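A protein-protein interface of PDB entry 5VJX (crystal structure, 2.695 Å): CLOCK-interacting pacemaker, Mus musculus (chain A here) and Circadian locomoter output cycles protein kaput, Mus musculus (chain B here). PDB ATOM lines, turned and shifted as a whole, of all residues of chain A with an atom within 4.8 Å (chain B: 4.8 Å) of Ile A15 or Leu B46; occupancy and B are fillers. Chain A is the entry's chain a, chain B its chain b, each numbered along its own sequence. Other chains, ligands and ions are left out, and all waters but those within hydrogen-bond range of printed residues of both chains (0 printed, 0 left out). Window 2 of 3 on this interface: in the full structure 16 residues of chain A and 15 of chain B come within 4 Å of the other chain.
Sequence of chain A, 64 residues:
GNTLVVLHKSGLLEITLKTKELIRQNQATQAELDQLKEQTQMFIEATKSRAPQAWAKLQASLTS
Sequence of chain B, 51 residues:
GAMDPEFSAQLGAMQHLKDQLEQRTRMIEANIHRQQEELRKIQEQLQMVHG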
ATOM      1  N   GLY A  11     -18.140  19.437  24.540  1.00  0.00           N
ATOM      2  CA  GLY A  11     -17.299  18.407  25.122  1.00  0.00           C
ATOM      3  C   GLY A  11     -15.835  18.646  25.420  1.00  0.00           C
ATOM      4  O   GLY A  11     -15.000  17.815  25.093  1.00  0.00           O
ATOM      5  N   LEU A  12     -15.525  19.746  26.095  1.00  0.00           N
ATOM      6  CA  LEU A  12     -14.171  19.938  26.593  1.00  0.00           C
ATOM      7  C   LEU A  12     -14.074  19.354  28.001  1.00  0.00           C
ATOM      8  O   LEU A  12     -12.989  19.198  28.557  1.00  0.00           O
ATOM      9  CB  LEU A  12     -13.805  21.419  26.626  1.00  0.00           C
ATOM     10  CG  LEU A  12     -13.566  22.128  25.302  1.00  0.00           C
ATOM     11  CD1 LEU A  12     -13.253  23.587  25.529  1.00  0.00           C
ATOM     12  CD2 LEU A  12     -12.415  21.463  24.617  1.00  0.00           C
ATOM     13  N   LEU A  13     -15.221  18.995  28.559  1.00  0.00           N
ATOM     14  CA  LEU A  13     -15.259  18.435  29.889  1.00  0.00           C
ATOM     15  C   LEU A  13     -14.657  17.055  29.837  1.00  0.00           C
ATOM     16  O   LEU A  13     -13.701  16.741  30.546  1.00  0.00           O
ATOM     17  CB  LEU A  13     -16.692  18.386  30.415  1.00  0.00           C
ATOM     18  CG  LEU A  13     -16.860  17.962  31.872  1.00  0.00           C
ATOM     19  CD1 LEU A  13     -16.101  18.911  32.760  1.00  0.00           C
ATOM     20  CD2 LEU A  13     -18.321  17.944  32.250  1.00  0.00           C
ATOM     21  N   GLU A  14     -15.221  16.252  28.947  1.00  0.00           N
ATOM     22  CA  GLU A  14     -14.795  14.885  28.704  1.00  0.00           C
ATOM     23  C   GLU A  14     -13.321  14.830  28.357  1.00  0.00           C
ATOM     24  O   GLU A  14     -12.582  13.983  28.853  1.00  0.00           O
ATOM     25  CB  GLU A  14     -15.651  14.276  27.598  1.00  0.00           C
ATOM     26  CG  GLU A  14     -15.348  12.841  27.262  1.00  0.00           C
ATOM     27  CD  GLU A  14     -16.362  12.268  26.300  1.00  0.00           C
ATOM     28  OE1 GLU A  14     -17.345  12.971  25.987  1.00  0.00           O
ATOM     29  OE2 GLU A  14     -16.179  11.121  25.853  1.00  0.00           O
ATOM     30  N   ILE A  15     -12.902  15.739  27.492  1.00  0.00           N
ATOM     31  CA  ILE A  15     -11.517  15.827  27.088  1.00  0.00           C
ATOM     32  C   ILE A  15     -10.610  16.161  28.262  1.00  0.00           C
ATOM     33  O   ILE A  15      -9.549  15.569  28.410  1.00  0.00           O
ATOM     34  CB  ILE A  15     -11.334  16.894  26.014  1.00  0.00           C
ATOM     35  CG1 ILE A  15     -12.061  16.499  24.742  1.00  0.00           C
ATOM     36  CG2 ILE A  15      -9.872  17.117  25.741  1.00  0.00           C
ATOM     37  CD1 ILE A  15     -12.089  17.582  23.738  1.00  0.00           C
ATOM     38  N   THR A  16     -11.033  17.104  29.104  1.00  0.00           N
ATOM     39  CA  THR A  16     -10.226  17.501  30.255  1.00  0.00           C
ATOM     40  C   THR A  16     -10.027  16.355  31.215  1.00  0.00           C
ATOM     41  O   THR A  16      -8.931  16.126  31.726  1.00  0.00           O
ATOM     42  CB  THR A  16     -10.861  18.648  31.033  1.00  0.00           C
ATOM     43  OG1 THR A  16     -11.095  19.751  30.160  1.00  0.00           O
ATOM     44  CG2 THR A  16      -9.933  19.092  32.131  1.00  0.00           C
ATOM     45  N   LEU A  17     -11.105  15.634  31.456  1.00  0.00           N
ATOM     46  CA  LEU A  17     -11.080  14.510  32.365  1.00  0.00           C
ATOM     47  C   LEU A  17     -10.259  13.329  31.865  1.00  0.00           C
ATOM     48  O   LEU A  17      -9.436  12.777  32.601  1.00  0.00           O
ATOM     49  CB  LEU A  17     -12.501  14.104  32.622  1.00  0.00           C
ATOM     50  CG  LEU A  17     -13.264  15.152  33.427  1.00  0.00           C
ATOM     51  CD1 LEU A  17     -14.717  15.148  33.045  1.00  0.00           C
ATOM     52  CD2 LEU A  17     -13.122  14.883  34.908  1.00  0.00           C
ATOM     53  N   LYS A  18     -10.488  12.937  30.613  1.00  0.00           N
ATOM     54  CA  LYS A  18      -9.702  11.870  29.995  1.00  0.00           C
ATOM     55  C   LYS A  18      -8.226  12.260  29.941  1.00  0.00           C
ATOM     56  O   LYS A  18      -7.361  11.412  30.084  1.00  0.00           O
ATOM     57  CB  LYS A  18     -10.234  11.498  28.606  1.00  0.00           C
ATOM     58  CG  LYS A  18     -11.594  10.815  28.673  1.00  0.00           C
ATOM     59  CD  LYS A  18     -12.148  10.339  27.341  1.00  0.00           C
ATOM     60  CE  LYS A  18     -11.317   9.171  26.821  1.00  0.00           C
ATOM     61  NZ  LYS A  18     -11.394   7.959  27.695  1.00  0.00           N
ATOM     62  N   THR A  19      -7.944  13.543  29.719  1.00  0.00           N
ATOM     63  CA  THR A  19      -6.573  14.048  29.669  1.00  0.00           C
ATOM     64  C   THR A  19      -5.897  14.011  31.048  1.00  0.00           C
ATOM     65  O   THR A  19      -4.748  13.620  31.159  1.00  0.00           O
ATOM     66  CB  THR A  19      -6.524  15.481  29.107  1.00  0.00           C
ATOM     67  OG1 THR A  19      -6.945  15.474  27.742  1.00  0.00           O
ATOM     68  CG2 THR A  19      -5.130  16.034  29.161  1.00  0.00           C
ATOM     69  N   ILE B  42      -7.970  10.979  22.335  1.00  0.00           N
ATOM     70  CA  ILE B  42      -8.104  12.317  22.897  1.00  0.00           C
ATOM     71  C   ILE B  42      -7.792  13.400  21.859  1.00  0.00           C
ATOM     72  O   ILE B  42      -8.516  14.372  21.742  1.00  0.00           O
ATOM     73  CB  ILE B  42      -7.204  12.487  24.110  1.00  0.00           C
ATOM     74  CG1 ILE B  42      -7.662  11.566  25.231  1.00  0.00           C
ATOM     75  CG2 ILE B  42      -7.198  13.921  24.582  1.00  0.00           C
ATOM     76  CD1 ILE B  42      -6.750  11.574  26.411  1.00  0.00           C
ATOM     77  N   GLN B  43      -6.720  13.216  21.098  1.00  0.00           N
ATOM     78  CA  GLN B  43      -6.321  14.162  20.058  1.00  0.00           C
ATOM     79  C   GLN B  43      -7.380  14.278  18.949  1.00  0.00           C
ATOM     80  O   GLN B  43      -7.608  15.357  18.388  1.00  0.00           O
ATOM     81  CB  GLN B  43      -4.986  13.718  19.472  1.00  0.00           C
ATOM     82  CG  GLN B  43      -3.810  13.925  20.396  1.00  0.00           C
ATOM     83  CD  GLN B  43      -2.509  13.374  19.835  1.00  0.00           C
ATOM     84  OE1 GLN B  43      -2.492  12.341  19.163  1.00  0.00           O
ATOM     85  NE2 GLN B  43      -1.411  14.056  20.120  1.00  0.00           N
ATOM     86  N   GLU B  44      -8.046  13.161  18.666  1.00  0.00           N
ATOM     87  CA  GLU B  44      -9.154  13.119  17.709  1.00  0.00           C
ATOM     88  C   GLU B  44     -10.329  13.940  18.185  1.00  0.00           C
ATOM     89  O   GLU B  44     -10.772  14.877  17.531  1.00  0.00           O
ATOM     90  CB  GLU B  44      -9.635  11.688  17.488  1.00  0.00           C
ATOM     91  CG  GLU B  44      -8.762  10.874  16.594  1.00  0.00           C
ATOM     92  CD  GLU B  44      -9.243   9.454  16.429  1.00  0.00           C
ATOM     93  OE1 GLU B  44     -10.269   9.098  17.042  1.00  0.00           O
ATOM     94  OE2 GLU B  44      -8.585   8.691  15.691  1.00  0.00           O
ATOM     95  N   GLN B  45     -10.854  13.521  19.325  1.00  0.00           N
ATOM     96  CA  GLN B  45     -11.910  14.222  20.041  1.00  0.00           C
ATOM     97  C   GLN B  45     -11.637  15.722  20.188  1.00  0.00           C
ATOM     98  O   GLN B  45     -12.554  16.533  20.231  1.00  0.00           O
ATOM     99  CB  GLN B  45     -12.120  13.566  21.403  1.00  0.00           C
ATOM    100  CG  GLN B  45     -13.296  14.099  22.175  1.00  0.00           C
ATOM    101  CD  GLN B  45     -13.656  13.192  23.320  1.00  0.00           C
ATOM    102  OE1 GLN B  45     -13.011  12.165  23.544  1.00  0.00           O
ATOM    103  NE2 GLN B  45     -14.694  13.559  24.053  1.00  0.00           N
ATOM    104  N   LEU B  46     -10.364  16.081  20.275  1.00  0.00           N
ATOM    105  CA  LEU B  46      -9.961  17.458  20.489  1.00  0.00           C
ATOM    106  C   LEU B  46      -9.891  18.202  19.169  1.00  0.00           C
ATOM    107  O   LEU B  46     -10.028  19.419  19.135  1.00  0.00           O
ATOM    108  CB  LEU B  46      -8.601  17.489  21.174  1.00  0.00           C
ATOM    109  CG  LEU B  46      -8.034  18.741  21.811  1.00  0.00           C
ATOM    110  CD1 LEU B  46      -8.951  19.220  22.891  1.00  0.00           C
ATOM    111  CD2 LEU B  46      -6.697  18.390  22.397  1.00  0.00           C
ATOM    112  N   GLN B  47      -9.698  17.474  18.074  1.00  0.00           N
ATOM    113  CA  GLN B  47      -9.739  18.114  16.760  1.00  0.00           C
ATOM    114  C   GLN B  47     -11.167  18.511  16.367  1.00  0.00           C
ATOM    115  O   GLN B  47     -11.362  19.311  15.458  1.00  0.00           O
ATOM    116  CB  GLN B  47      -9.136  17.208  15.679  1.00  0.00           C
ATOM    117  CG  GLN B  47      -8.837  17.948  14.368  1.00  0.00           C
ATOM    118  CD  GLN B  47      -8.339  17.041  13.260  1.00  0.00           C
ATOM    119  OE1 GLN B  47      -7.795  15.969  13.522  1.00  0.00           O
ATOM    120  NE2 GLN B  47      -8.486  17.488  12.011  1.00  0.00           N
ATOM    121  N   MET B  48     -12.162  17.977  17.065  1.00  0.00           N
ATOM    122  CA  MET B  48     -13.550  18.220  16.689  1.00  0.00           C
ATOM    123  C   MET B  48     -14.237  19.286  17.533  1.00  0.00           C
ATOM    124  O   MET B  48     -15.457  19.394  17.512  1.00  0.00           O
ATOM    125  CB  MET B  48     -14.353  16.922  16.768  1.00  0.00           C
ATOM    126  CG  MET B  48     -13.754  15.761  15.997  1.00  0.00           C
ATOM    127  SD  MET B  48     -14.750  15.302  14.395  1.00  0.00           S
ATOM    128  CE  MET B  48     -14.115  16.708  13.209  1.00  0.00           C
ATOM    129  N   VAL B  49     -13.463  20.072  18.273  1.00  0.00           N
ATOM    130  CA  VAL B  49     -14.033  21.150  19.079  1.00  0.00           C
ATOM    131  C   VAL B  49     -13.724  22.520  18.485  1.00  0.00           C
ATOM    132  O   VAL B  49     -12.569  22.887  18.300  1.00  0.00           O
ATOM    133  CB  VAL B  49     -13.529  21.108  20.529  1.00  0.00           C
ATOM    134  CG1 VAL B  49     -14.032  22.316  21.298  1.00  0.00           C
ATOM    135  CG2 VAL B  49     -13.971  19.825  21.205  1.00  0.00           C
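Ile A15 touches just these residues of chain B: Gln B45, Leu B46 and Val B49. Of chain A, only Ile A15 (3.6 Å) comes within 4 Å of Leu B46. Printed residues of chain B within 4 Å of Leu A12: Val B49. Printed residues of chain B within 4 Å of Thr A19: Ile B42. Leu A17 touches none of the printed residues of chain B. The nearest residue of chain B that does not touch Ile A15 is Ile B42 (4.3 Å). The nearest residue of chain A that does not touch Leu B46 is Leu A12 (4.5 Å). The nearest printed residue of chain B that does not touch Glu A14 is Ile B42 (6.6 Å).
OE1 of Glu A14 sits close to NE2 of Gln B45.
Hydrophobic or aromatic side chains of chain B within 4 Å of the printed part of chain A: Ile B42, Leu B46 and Val B49. Of the 9 printed residues of chain A, 5 touch a printed residue of chain B. Among the printed residues, no Asp or Glu carboxylate lies within 4 Å of a Lys or Arg side-chain nitrogen of the other chain.
OG1 of Thr A16 is in hydrogen-bond range of O of Leu A12 (2.5 Å). The backbone carbonyl oxygen (O) of Ile A15 sits at hydrogen-bond distance from the side-chain hydroxyl (OG1) of Thr A19 (2.7 Å).
Among the printed residues, merely in contact across the chains: Leu A12 with Val B49 (3.8 Å), Ile A15 with Gln B45 (3.7 Å), Ile A15 with Leu B46 (3.6 Å), Ile A15 with Val B49 (3.9 Å), Lys A18 with Ile B42 (3.7 Å) and Thr A19 with Ile B42 (3.5 Å).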
